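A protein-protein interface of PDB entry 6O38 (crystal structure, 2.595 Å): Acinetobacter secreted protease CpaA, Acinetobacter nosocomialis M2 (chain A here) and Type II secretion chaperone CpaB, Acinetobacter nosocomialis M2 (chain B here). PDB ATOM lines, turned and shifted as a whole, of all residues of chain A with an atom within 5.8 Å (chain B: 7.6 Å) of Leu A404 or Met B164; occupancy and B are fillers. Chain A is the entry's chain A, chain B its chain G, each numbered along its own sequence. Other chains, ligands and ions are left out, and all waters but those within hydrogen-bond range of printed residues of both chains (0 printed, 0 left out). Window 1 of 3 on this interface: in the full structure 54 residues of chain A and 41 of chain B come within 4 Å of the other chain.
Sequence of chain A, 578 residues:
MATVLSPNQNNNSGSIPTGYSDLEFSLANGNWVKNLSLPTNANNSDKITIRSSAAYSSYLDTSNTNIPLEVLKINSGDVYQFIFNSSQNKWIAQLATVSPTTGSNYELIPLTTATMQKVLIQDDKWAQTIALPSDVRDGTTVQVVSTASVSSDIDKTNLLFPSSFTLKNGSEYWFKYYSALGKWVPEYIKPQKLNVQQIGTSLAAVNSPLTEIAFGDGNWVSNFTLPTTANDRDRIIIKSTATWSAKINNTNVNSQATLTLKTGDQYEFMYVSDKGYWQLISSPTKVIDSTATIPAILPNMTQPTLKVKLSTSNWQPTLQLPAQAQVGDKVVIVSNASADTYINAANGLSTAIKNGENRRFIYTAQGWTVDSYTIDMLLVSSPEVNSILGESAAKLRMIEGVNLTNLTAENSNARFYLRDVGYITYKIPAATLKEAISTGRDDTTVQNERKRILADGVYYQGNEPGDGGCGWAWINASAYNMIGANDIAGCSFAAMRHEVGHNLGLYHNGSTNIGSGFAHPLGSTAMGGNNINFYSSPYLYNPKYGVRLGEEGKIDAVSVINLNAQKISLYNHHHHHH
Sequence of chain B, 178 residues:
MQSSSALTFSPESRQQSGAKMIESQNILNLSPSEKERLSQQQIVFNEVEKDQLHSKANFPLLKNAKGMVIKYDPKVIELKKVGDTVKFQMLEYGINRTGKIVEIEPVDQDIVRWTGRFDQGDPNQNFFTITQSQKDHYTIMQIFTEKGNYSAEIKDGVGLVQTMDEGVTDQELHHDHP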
ATOM      1  N   ILE A 399      32.594  17.177  16.601  1.00  0.00           N
ATOM      2  CA  ILE A 399      33.580  16.866  15.569  1.00  0.00           C
ATOM      3  C   ILE A 399      32.905  16.732  14.210  1.00  0.00           C
ATOM      4  O   ILE A 399      33.411  17.231  13.197  1.00  0.00           O
ATOM      5  CB  ILE A 399      34.364  15.594  15.944  1.00  0.00           C
ATOM      6  CG1 ILE A 399      35.290  15.871  17.131  1.00  0.00           C
ATOM      7  CG2 ILE A 399      35.163  15.084  14.756  1.00  0.00           C
ATOM      8  CD1 ILE A 399      36.146  17.110  16.963  1.00  0.00           C
ATOM      9  N   GLU A 400      31.750  16.063  14.164  1.00  0.00           N
ATOM     10  CA  GLU A 400      31.012  15.958  12.910  1.00  0.00           C
ATOM     11  C   GLU A 400      30.552  17.326  12.421  1.00  0.00           C
ATOM     12  O   GLU A 400      30.459  17.553  11.210  1.00  0.00           O
ATOM     13  CB  GLU A 400      29.816  15.020  13.077  1.00  0.00           C
ATOM     14  CG  GLU A 400      30.194  13.580  13.390  1.00  0.00           C
ATOM     15  CD  GLU A 400      31.181  12.995  12.393  1.00  0.00           C
ATOM     16  OE1 GLU A 400      31.066  13.297  11.186  1.00  0.00           O
ATOM     17  OE2 GLU A 400      32.073  12.233  12.820  1.00  0.00           O
ATOM     18  N   GLY A 401      30.258  18.243  13.346  1.00  0.00           N
ATOM     19  CA  GLY A 401      29.973  19.611  12.948  1.00  0.00           C
ATOM     20  C   GLY A 401      31.176  20.294  12.326  1.00  0.00           C
ATOM     21  O   GLY A 401      31.039  21.075  11.382  1.00  0.00           O
ATOM     22  N   VAL A 402      32.370  20.014  12.852  1.00  0.00           N
ATOM     23  CA  VAL A 402      33.589  20.583  12.284  1.00  0.00           C
ATOM     24  C   VAL A 402      33.846  20.013  10.894  1.00  0.00           C
ATOM     25  O   VAL A 402      34.167  20.748   9.954  1.00  0.00           O
ATOM     26  CB  VAL A 402      34.784  20.336  13.224  1.00  0.00           C
ATOM     27  CG1 VAL A 402      36.066  20.874  12.606  1.00  0.00           C
ATOM     28  CG2 VAL A 402      34.537  20.973  14.581  1.00  0.00           C
ATOM     29  N   ASN A 403      33.708  18.693  10.746  1.00  0.00           N
ATOM     30  CA  ASN A 403      33.963  18.057   9.456  1.00  0.00           C
ATOM     31  C   ASN A 403      32.993  18.551   8.390  1.00  0.00           C
ATOM     32  O   ASN A 403      33.379  18.744   7.231  1.00  0.00           O
ATOM     33  CB  ASN A 403      33.882  16.537   9.596  1.00  0.00           C
ATOM     34  CG  ASN A 403      34.991  15.972  10.458  1.00  0.00           C
ATOM     35  OD1 ASN A 403      36.103  16.499  10.483  1.00  0.00           O
ATOM     36  ND2 ASN A 403      34.693  14.895  11.175  1.00  0.00           N
ATOM     37  N   LEU A 404      31.728  18.758   8.761  1.00  0.00           N
ATOM     38  CA  LEU A 404      30.752  19.242   7.790  1.00  0.00           C
ATOM     39  C   LEU A 404      31.043  20.681   7.386  1.00  0.00           C
ATOM     40  O   LEU A 404      30.854  21.054   6.221  1.00  0.00           O
ATOM     41  CB  LEU A 404      29.339  19.116   8.358  1.00  0.00           C
ATOM     42  CG  LEU A 404      28.208  19.549   7.424  1.00  0.00           C
ATOM     43  CD1 LEU A 404      28.135  18.631   6.216  1.00  0.00           C
ATOM     44  CD2 LEU A 404      26.883  19.571   8.164  1.00  0.00           C
ATOM     45  N   THR A 405      31.501  21.504   8.331  1.00  0.00           N
ATOM     46  CA  THR A 405      31.873  22.876   8.001  1.00  0.00           C
ATOM     47  C   THR A 405      33.041  22.906   7.022  1.00  0.00           C
ATOM     48  O   THR A 405      33.020  23.648   6.033  1.00  0.00           O
ATOM     49  CB  THR A 405      32.215  23.651   9.273  1.00  0.00           C
ATOM     50  OG1 THR A 405      31.132  23.545  10.204  1.00  0.00           O
ATOM     51  CG2 THR A 405      32.456  25.119   8.951  1.00  0.00           C
ATOM     52  N   ASN A 406      34.075  22.103   7.287  1.00  0.00           N
ATOM     53  CA  ASN A 406      35.228  22.066   6.393  1.00  0.00           C
ATOM     54  C   ASN A 406      34.849  21.512   5.024  1.00  0.00           C
ATOM     55  O   ASN A 406      35.389  21.949   4.001  1.00  0.00           O
ATOM     56  CB  ASN A 406      36.355  21.241   7.014  1.00  0.00           C
ATOM     57  CG  ASN A 406      36.960  21.908   8.232  1.00  0.00           C
ATOM     58  OD1 ASN A 406      36.889  23.127   8.387  1.00  0.00           O
ATOM     59  ND2 ASN A 406      37.565  21.109   9.104  1.00  0.00           N
ATOM     60  N   LEU A 407      33.929  20.546   4.985  1.00  0.00           N
ATOM     61  CA  LEU A 407      33.458  20.034   3.703  1.00  0.00           C
ATOM     62  C   LEU A 407      32.675  21.098   2.942  1.00  0.00           C
ATOM     63  O   LEU A 407      32.843  21.249   1.725  1.00  0.00           O
ATOM     64  CB  LEU A 407      32.602  18.786   3.916  1.00  0.00           C
ATOM     65  CG  LEU A 407      31.922  18.225   2.665  1.00  0.00           C
ATOM     66  CD1 LEU A 407      32.957  17.682   1.691  1.00  0.00           C
ATOM     67  CD2 LEU A 407      30.909  17.153   3.030  1.00  0.00           C
ATOM     68  N   THR A 408      31.815  21.842   3.642  1.00  0.00           N
ATOM     69  CA  THR A 408      31.068  22.917   2.998  1.00  0.00           C
ATOM     70  C   THR A 408      32.000  24.013   2.498  1.00  0.00           C
ATOM     71  O   THR A 408      31.832  24.524   1.384  1.00  0.00           O
ATOM     72  CB  THR A 408      30.037  23.493   3.971  1.00  0.00           C
ATOM     73  OG1 THR A 408      29.152  22.452   4.403  1.00  0.00           O
ATOM     74  CG2 THR A 408      29.227  24.595   3.305  1.00  0.00           C
ATOM     75  N   ALA A 409      32.990  24.391   3.312  1.00  0.00           N
ATOM     76  CA  ALA A 409      33.933  25.425   2.903  1.00  0.00           C
ATOM     77  C   ALA A 409      34.749  24.987   1.693  1.00  0.00           C
ATOM     78  O   ALA A 409      34.966  25.772   0.763  1.00  0.00           O
ATOM     79  CB  ALA A 409      34.856  25.784   4.068  1.00  0.00           C
ATOM     80  N   SER A 492      20.746  20.176  15.149  1.00  0.00           N
ATOM     81  CA  SER A 492      21.632  19.064  14.846  1.00  0.00           C
ATOM     82  C   SER A 492      23.052  19.588  14.638  1.00  0.00           C
ATOM     83  O   SER A 492      23.328  20.783  14.762  1.00  0.00           O
ATOM     84  CB  SER A 492      21.137  18.296  13.618  1.00  0.00           C
ATOM     85  OG  SER A 492      21.468  18.977  12.419  1.00  0.00           O
ATOM     86  N   PHE A 493      23.970  18.675  14.311  1.00  0.00           N
ATOM     87  CA  PHE A 493      25.360  19.066  14.110  1.00  0.00           C
ATOM     88  C   PHE A 493      25.569  19.882  12.840  1.00  0.00           C
ATOM     89  O   PHE A 493      26.667  20.415  12.644  1.00  0.00           O
ATOM     90  CB  PHE A 493      26.266  17.832  14.092  1.00  0.00           C
ATOM     91  CG  PHE A 493      25.976  16.875  12.969  1.00  0.00           C
ATOM     92  CD1 PHE A 493      25.054  15.854  13.133  1.00  0.00           C
ATOM     93  CD2 PHE A 493      26.632  16.990  11.754  1.00  0.00           C
ATOM     94  CE1 PHE A 493      24.789  14.971  12.106  1.00  0.00           C
ATOM     95  CE2 PHE A 493      26.369  16.110  10.722  1.00  0.00           C
ATOM     96  CZ  PHE A 493      25.448  15.099  10.899  1.00  0.00           C
ATOM     97  N   ALA A 494      24.557  19.993  11.980  1.00  0.00           N
ATOM     98  CA  ALA A 494      24.648  20.858  10.812  1.00  0.00           C
ATOM     99  C   ALA A 494      24.501  22.333  11.159  1.00  0.00           C
ATOM    100  O   ALA A 494      24.658  23.181  10.275  1.00  0.00           O
ATOM    101  CB  ALA A 494      23.587  20.465   9.780  1.00  0.00           C
ATOM    102  N   ARG A 497      28.148  24.912  10.986  1.00  0.00           N
ATOM    103  CA  ARG A 497      28.503  25.635   9.771  1.00  0.00           C
ATOM    104  C   ARG A 497      27.592  26.830   9.537  1.00  0.00           C
ATOM    105  O   ARG A 497      27.978  27.759   8.817  1.00  0.00           O
ATOM    106  CB  ARG A 497      28.461  24.700   8.560  1.00  0.00           C
ATOM    107  CG  ARG A 497      27.067  24.244   8.158  1.00  0.00           C
ATOM    108  CD  ARG A 497      27.106  23.487   6.841  1.00  0.00           C
ATOM    109  NE  ARG A 497      25.788  23.009   6.434  1.00  0.00           N
ATOM    110  CZ  ARG A 497      25.576  22.202   5.399  1.00  0.00           C
ATOM    111  NH1 ARG A 497      26.597  21.779   4.667  1.00  0.00           N
ATOM    112  NH2 ARG A 497      24.344  21.814   5.099  1.00  0.00           N
ATOM    113  N   GLY A 529      19.017  28.437   4.126  1.00  0.00           N
ATOM    114  CA  GLY A 529      18.195  27.249   4.245  1.00  0.00           C
ATOM    115  C   GLY A 529      18.972  26.020   4.669  1.00  0.00           C
ATOM    116  O   GLY A 529      18.426  25.148   5.350  1.00  0.00           O
ATOM    117  N   ASN A 530      20.242  25.938   4.271  1.00  0.00           N
ATOM    118  CA  ASN A 530      21.197  24.986   4.843  1.00  0.00           C
ATOM    119  C   ASN A 530      20.837  23.533   4.525  1.00  0.00           C
ATOM    120  O   ASN A 530      20.885  22.666   5.398  1.00  0.00           O
ATOM    121  CB  ASN A 530      21.328  25.192   6.357  1.00  0.00           C
ATOM    122  CG  ASN A 530      22.570  24.543   6.931  1.00  0.00           C
ATOM    123  OD1 ASN A 530      23.561  24.345   6.230  1.00  0.00           O
ATOM    124  ND2 ASN A 530      22.521  24.204   8.215  1.00  0.00           N
ATOM    125  N   ASN A 531      20.475  23.253   3.271  1.00  0.00           N
ATOM    126  CA  ASN A 531      20.192  21.884   2.858  1.00  0.00           C
ATOM    127  C   ASN A 531      21.116  21.372   1.759  1.00  0.00           C
ATOM    128  O   ASN A 531      20.926  20.243   1.290  1.00  0.00           O
ATOM    129  CB  ASN A 531      18.725  21.740   2.420  1.00  0.00           C
ATOM    130  CG  ASN A 531      18.337  22.701   1.312  1.00  0.00           C
ATOM    131  OD1 ASN A 531      19.186  23.211   0.581  1.00  0.00           O
ATOM    132  ND2 ASN A 531      17.040  22.952   1.183  1.00  0.00           N
ATOM    133  N   ILE A 532      22.105  22.158   1.334  1.00  0.00           N
ATOM    134  CA  ILE A 532      23.157  21.690   0.442  1.00  0.00           C
ATOM    135  C   ILE A 532      24.493  22.157   1.001  1.00  0.00           C
ATOM    136  O   ILE A 532      24.569  23.149   1.733  1.00  0.00           O
ATOM    137  CB  ILE A 532      22.972  22.179  -1.015  1.00  0.00           C
ATOM    138  CG1 ILE A 532      23.033  23.704  -1.091  1.00  0.00           C
ATOM    139  CG2 ILE A 532      21.668  21.656  -1.604  1.00  0.00           C
ATOM    140  CD1 ILE A 532      22.986  24.245  -2.502  1.00  0.00           C
ATOM    141  N   ASN A 533      25.553  21.431   0.653  1.00  0.00           N
ATOM    142  CA  ASN A 533      26.870  21.643   1.254  1.00  0.00           C
ATOM    143  C   ASN A 533      27.638  22.742   0.516  1.00  0.00           C
ATOM    144  O   ASN A 533      28.697  22.518  -0.072  1.00  0.00           O
ATOM    145  CB  ASN A 533      27.654  20.336   1.269  1.00  0.00           C
ATOM    146  CG  ASN A 533      26.925  19.228   2.001  1.00  0.00           C
ATOM    147  OD1 ASN A 533      26.179  19.477   2.947  1.00  0.00           O
ATOM    148  ND2 ASN A 533      27.134  17.993   1.560  1.00  0.00           N
ATOM    149  N   MET B 141      25.366   9.665  11.153  1.00  0.00           N
ATOM    150  CA  MET B 141      25.516   9.345   9.737  1.00  0.00           C
ATOM    151  C   MET B 141      25.411  10.583   8.859  1.00  0.00           C
ATOM    152  O   MET B 141      24.537  11.426   9.055  1.00  0.00           O
ATOM    153  CB  MET B 141      24.464   8.328   9.297  1.00  0.00           C
ATOM    154  CG  MET B 141      24.518   7.018  10.044  1.00  0.00           C
ATOM    155  SD  MET B 141      23.299   5.714   9.278  1.00  0.00           S
ATOM    156  CE  MET B 141      23.411   4.385  10.688  1.00  0.00           C
ATOM    157  N   GLN B 142      26.310  10.682   7.883  1.00  0.00           N
ATOM    158  CA  GLN B 142      26.282  11.740   6.880  1.00  0.00           C
ATOM    159  C   GLN B 142      26.068  11.086   5.523  1.00  0.00           C
ATOM    160  O   GLN B 142      26.945  10.370   5.031  1.00  0.00           O
ATOM    161  CB  GLN B 142      27.577  12.551   6.894  1.00  0.00           C
ATOM    162  CG  GLN B 142      27.887  13.221   8.220  1.00  0.00           C
ATOM    163  CD  GLN B 142      29.181  14.008   8.176  1.00  0.00           C
ATOM    164  OE1 GLN B 142      29.758  14.218   7.109  1.00  0.00           O
ATOM    165  NE2 GLN B 142      29.648  14.445   9.340  1.00  0.00           N
ATOM    166  N   ILE B 143      24.904  11.318   4.928  1.00  0.00           N
ATOM    167  CA  ILE B 143      24.549  10.742   3.636  1.00  0.00           C
ATOM    168  C   ILE B 143      24.498  11.887   2.633  1.00  0.00           C
ATOM    169  O   ILE B 143      23.609  12.745   2.700  1.00  0.00           O
ATOM    170  CB  ILE B 143      23.219   9.981   3.697  1.00  0.00           C
ATOM    171  CG1 ILE B 143      23.266   8.943   4.821  1.00  0.00           C
ATOM    172  CG2 ILE B 143      22.921   9.316   2.362  1.00  0.00           C
ATOM    173  CD1 ILE B 143      21.909   8.471   5.284  1.00  0.00           C
ATOM    174  N   PHE B 144      25.448  11.901   1.701  1.00  0.00           N
ATOM    175  CA  PHE B 144      25.585  12.976   0.723  1.00  0.00           C
ATOM    176  C   PHE B 144      25.282  12.424  -0.665  1.00  0.00           C
ATOM    177  O   PHE B 144      26.081  11.669  -1.228  1.00  0.00           O
ATOM    178  CB  PHE B 144      26.985  13.583   0.780  1.00  0.00           C
ATOM    179  CG  PHE B 144      27.335  14.170   2.117  1.00  0.00           C
ATOM    180  CD1 PHE B 144      26.477  15.055   2.747  1.00  0.00           C
ATOM    181  CD2 PHE B 144      28.523  13.834   2.746  1.00  0.00           C
ATOM    182  CE1 PHE B 144      26.797  15.596   3.979  1.00  0.00           C
ATOM    183  CE2 PHE B 144      28.848  14.372   3.978  1.00  0.00           C
ATOM    184  CZ  PHE B 144      27.984  15.253   4.594  1.00  0.00           C
ATOM    185  N   GLY B 148      20.142  15.376  -2.356  1.00  0.00           N
ATOM    186  CA  GLY B 148      20.010  15.999  -1.052  1.00  0.00           C
ATOM    187  C   GLY B 148      20.957  15.373  -0.053  1.00  0.00           C
ATOM    188  O   GLY B 148      21.556  14.326  -0.287  1.00  0.00           O
ATOM    189  N   ASN B 149      21.080  16.044   1.090  1.00  0.00           N
ATOM    190  CA  ASN B 149      21.973  15.635   2.165  1.00  0.00           C
ATOM    191  C   ASN B 149      21.160  15.317   3.411  1.00  0.00           C
ATOM    192  O   ASN B 149      20.245  16.063   3.773  1.00  0.00           O
ATOM    193  CB  ASN B 149      22.996  16.730   2.467  1.00  0.00           C
ATOM    194  CG  ASN B 149      23.764  17.156   1.236  1.00  0.00           C
ATOM    195  OD1 ASN B 149      24.286  16.323   0.498  1.00  0.00           O
ATOM    196  ND2 ASN B 149      23.828  18.460   1.000  1.00  0.00           N
ATOM    197  N   TYR B 150      21.493  14.207   4.063  1.00  0.00           N
ATOM    198  CA  TYR B 150      20.708  13.711   5.183  1.00  0.00           C
ATOM    199  C   TYR B 150      21.619  13.337   6.342  1.00  0.00           C
ATOM    200  O   TYR B 150      22.661  12.703   6.149  1.00  0.00           O
ATOM    201  CB  TYR B 150      19.863  12.507   4.758  1.00  0.00           C
ATOM    202  CG  TYR B 150      19.047  12.782   3.518  1.00  0.00           C
ATOM    203  CD1 TYR B 150      17.798  13.382   3.602  1.00  0.00           C
ATOM    204  CD2 TYR B 150      19.538  12.462   2.261  1.00  0.00           C
ATOM    205  CE1 TYR B 150      17.056  13.646   2.468  1.00  0.00           C
ATOM    206  CE2 TYR B 150      18.805  12.723   1.121  1.00  0.00           C
ATOM    207  CZ  TYR B 150      17.564  13.312   1.229  1.00  0.00           C
ATOM    208  OH  TYR B 150      16.827  13.573   0.095  1.00  0.00           O
ATOM    209  N   SER B 151      21.219  13.740   7.543  1.00  0.00           N
ATOM    210  CA  SER B 151      21.942  13.437   8.767  1.00  0.00           C
ATOM    211  C   SER B 151      21.102  12.525   9.650  1.00  0.00           C
ATOM    212  O   SER B 151      19.880  12.686   9.740  1.00  0.00           O
ATOM    213  CB  SER B 151      22.292  14.718   9.527  1.00  0.00           C
ATOM    214  OG  SER B 151      21.121  15.435   9.882  1.00  0.00           O
ATOM    215  N   ALA B 152      21.760  11.569  10.300  1.00  0.00           N
ATOM    216  CA  ALA B 152      21.100  10.633  11.201  1.00  0.00           C
ATOM    217  C   ALA B 152      21.822  10.651  12.538  1.00  0.00           C
ATOM    218  O   ALA B 152      23.036  10.430  12.592  1.00  0.00           O
ATOM    219  CB  ALA B 152      21.082   9.217  10.616  1.00  0.00           C
ATOM    220  N   VAL B 161      16.424  10.774  11.357  1.00  0.00           N
ATOM    221  CA  VAL B 161      16.983  11.231  10.091  1.00  0.00           C
ATOM    222  C   VAL B 161      16.179  12.432   9.622  1.00  0.00           C
ATOM    223  O   VAL B 161      14.948  12.451   9.732  1.00  0.00           O
ATOM    224  CB  VAL B 161      16.988  10.125   9.019  1.00  0.00           C
ATOM    225  CG1 VAL B 161      18.277  10.176   8.216  1.00  0.00           C
ATOM    226  CG2 VAL B 161      16.824   8.769   9.663  1.00  0.00           C
ATOM    227  N   GLN B 162      16.878  13.433   9.098  1.00  0.00           N
ATOM    228  CA  GLN B 162      16.237  14.664   8.671  1.00  0.00           C
ATOM    229  C   GLN B 162      17.089  15.323   7.599  1.00  0.00           C
ATOM    230  O   GLN B 162      18.293  15.074   7.494  1.00  0.00           O
ATOM    231  CB  GLN B 162      16.038  15.628   9.848  1.00  0.00           C
ATOM    232  CG  GLN B 162      17.343  16.025  10.527  1.00  0.00           C
ATOM    233  CD  GLN B 162      17.132  16.906  11.743  1.00  0.00           C
ATOM    234  OE1 GLN B 162      16.097  16.836  12.403  1.00  0.00           O
ATOM    235  NE2 GLN B 162      18.120  17.740  12.045  1.00  0.00           N
ATOM    236  N   THR B 163      16.446  16.166   6.799  1.00  0.00           N
ATOM    237  CA  THR B 163      17.189  17.023   5.893  1.00  0.00           C
ATOM    238  C   THR B 163      17.919  18.091   6.698  1.00  0.00           C
ATOM    239  O   THR B 163      17.466  18.513   7.765  1.00  0.00           O
ATOM    240  CB  THR B 163      16.254  17.672   4.871  1.00  0.00           C
ATOM    241  OG1 THR B 163      14.897  17.325   5.174  1.00  0.00           O
ATOM    242  CG2 THR B 163      16.591  17.197   3.465  1.00  0.00           C
ATOM    243  N   MET B 164      19.063  18.522   6.180  1.00  0.00           N
ATOM    244  CA  MET B 164      19.951  19.402   6.935  1.00  0.00           C
ATOM    245  C   MET B 164      19.353  20.786   7.178  1.00  0.00           C
ATOM    246  O   MET B 164      19.868  21.555   7.991  1.00  0.00           O
ATOM    247  CB  MET B 164      21.297  19.523   6.219  1.00  0.00           C
ATOM    248  CG  MET B 164      21.986  18.183   6.019  1.00  0.00           C
ATOM    249  SD  MET B 164      23.893  18.224   6.412  1.00  0.00           S
ATOM    250  CE  MET B 164      24.248  16.306   6.350  1.00  0.00           C
ATOM    251  N   ASP B 165      18.263  21.105   6.473  1.00  0.00           N
ATOM    252  CA  ASP B 165      17.581  22.371   6.716  1.00  0.00           C
ATOM    253  C   ASP B 165      16.886  22.378   8.071  1.00  0.00           C
ATOM    254  O   ASP B 165      16.746  23.439   8.690  1.00  0.00           O
ATOM    255  CB  ASP B 165      16.574  22.655   5.600  1.00  0.00           C
ATOM    256  CG  ASP B 165      15.601  21.513   5.380  1.00  0.00           C
ATOM    257  OD1 ASP B 165      15.680  20.507   6.115  1.00  0.00           O
ATOM    258  OD2 ASP B 165      14.756  21.622   4.468  1.00  0.00           O
ATOM    259  N   GLU B 166      16.447  21.211   8.544  1.00  0.00           N
ATOM    260  CA  GLU B 166      15.885  21.085   9.882  1.00  0.00           C
ATOM    261  C   GLU B 166      16.935  21.208  10.976  1.00  0.00           C
ATOM    262  O   GLU B 166      16.569  21.319  12.151  1.00  0.00           O
ATOM    263  CB  GLU B 166      15.164  19.741  10.019  1.00  0.00           C
ATOM    264  CG  GLU B 166      13.983  19.560   9.079  1.00  0.00           C
ATOM    265  CD  GLU B 166      12.836  20.502   9.386  1.00  0.00           C
ATOM    266  OE1 GLU B 166      12.763  21.007  10.527  1.00  0.00           O
ATOM    267  OE2 GLU B 166      12.004  20.739   8.485  1.00  0.00           O
ATOM    268  N   GLY B 167      18.222  21.187  10.623  1.00  0.00           N
ATOM    269  CA  GLY B 167      19.271  21.126  11.622  1.00  0.00           C
ATOM    270  C   GLY B 167      19.489  22.411  12.393  1.00  0.00           C
ATOM    271  O   GLY B 167      20.127  22.380  13.451  1.00  0.00           O
ATOM    272  N   VAL B 168      18.986  23.536  11.895  1.00  0.00           N
ATOM    273  CA  VAL B 168      19.182  24.813  12.576  1.00  0.00           C
ATOM    274  C   VAL B 168      18.035  25.753  12.232  1.00  0.00           C
ATOM    275  O   VAL B 168      17.647  25.883  11.066  1.00  0.00           O
ATOM    276  CB  VAL B 168      20.546  25.446  12.225  1.00  0.00           C
ATOM    277  CG1 VAL B 168      20.676  25.676  10.725  1.00  0.00           C
ATOM    278  CG2 VAL B 168      20.744  26.746  12.994  1.00  0.00           C
ATOM    279  N   THR B 169      17.477  26.386  13.261  1.00  0.00           N
ATOM    280  CA  THR B 169      16.598  27.539  13.121  1.00  0.00           C
ATOM    281  C   THR B 169      17.040  28.574  14.143  1.00  0.00           C
ATOM    282  O   THR B 169      17.207  28.250  15.323  1.00  0.00           O
ATOM    283  CB  THR B 169      15.123  27.168  13.332  1.00  0.00           C
ATOM    284  OG1 THR B 169      15.000  26.322  14.481  1.00  0.00           O
ATOM    285  CG2 THR B 169      14.569  26.450  12.108  1.00  0.00           C
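The side-chain amide nitrogen (NE2) of Gln B142 lies within hydrogen-bond range of the side-chain carboxylate (OE1) of Glu A400 (2.6 Å).
The backbone carbonyl oxygen (O) of Gly B167 is in hydrogen-bond range of the backbone NH (N) of Ser A492 (2.9 Å).
The backbone carbonyl oxygen (O) of Asn A530 is in hydrogen-bond range of the backbone NH (N) of Asp B165 (3.2 Å).
ND2 of Asn B149 sits at hydrogen-bond distance from O of Asn A531, at 3.4 Å.
The side-chain amide nitrogen of Asn B149 is in hydrogen-bond range of the side-chain amide oxygen of Asn A533 (3.2 Å).
O of Asn A530 lies close to O of Met B164, at 3.0 Å.
The side-chain hydroxyl (OG1) of Thr A405 lies close to the backbone NH (N) of Arg A497, 3.4 Å away.
The side-chain hydroxyl of Thr A408 lies within hydrogen-bond range of the guanidinium group of Arg A497, 2.7 Å away.
The side-chain hydroxyl (OG) of Ser A492 sits close to the backbone NH (N) of Ala A494 (3.3 Å).
The side-chain amide oxygen (OD1) of Asn A530 lies within hydrogen-bond range of the guanidinium group (NE) of Arg A497, 2.6 Å away.
The backbone NH of Gln B162 lies within hydrogen-bond range of the backbone carbonyl oxygen of Ser B151 (3.2 Å).
OG1 of Thr B163 lies close to OD1 of Asp B165.
Leu A404 touches Met B164 (CD2 to SD, 3.7 Å).
NE2 of Gln B162 touches CB of Ser A492 (3.4 Å).
CE2 of Phe A493 touches NE2 of Gln B142, at 3.9 Å.
CB of Ser B151 touches CZ of Phe A493, 3.5 Å away.
Met B164 touches Arg A497 (SD to NH2, 3.8 Å).
O of Gly A529 touches CB of Asp B165 (3.1 Å).
Asn A530 touches Val B168 (ND2 to CG1, 3.4 Å).
Asn A531 touches Asp B165 (CB to CB, 3.9 Å).
Ile A532 touches Asn B149.
Asn A533 touches Phe B144 (ND2 to CD1, 3.2 Å).
Leu A404 touches just these residues of chain B: Phe B144 (3.8 Å) and Met B164 (3.7 Å).
Met B164 touches just these residues of chain A: Leu A404, Arg A497 and Asn A530.
Of the printed residues of chain B, Asn A533 touches Phe B144 (3.2 Å) and Asn B149 (3.2 Å).
Of the printed residues of chain B, Asn A530 touches Met B164, Asp B165 and Val B168.
Asn A406 touches none of the printed residues of chain B.
Tyr B150 touches none of the printed residues of chain A.
The nearest residue of chain B that does not touch Leu A404 is Gln B142 (4.8 Å).
The nearest residue of chain A that does not touch Met B164 is Ala A494 (4.1 Å).
Hydrophobic or aromatic side chains of chain A within 4 Å of the printed part of chain B: Leu A404, Leu A407 and Phe A493.
Printed residues of chain B that touch a printed residue of chain A: Gln B142, Phe B144, Asn B149, Ser B151, Gln B162, Met B164, Asp B165, Gly B167 and Val B168.
Hydrophobic or aromatic side chains of chain B within 4 Å of the printed part of chain A: Phe B144, Met B164 and Val B168.
Among the printed residues, 18 pairs touch across the chains.
Among the printed residues, no Asp or Glu carboxylate lies within 4 Å of a Lys or Arg side-chain nitrogen of the other chain.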
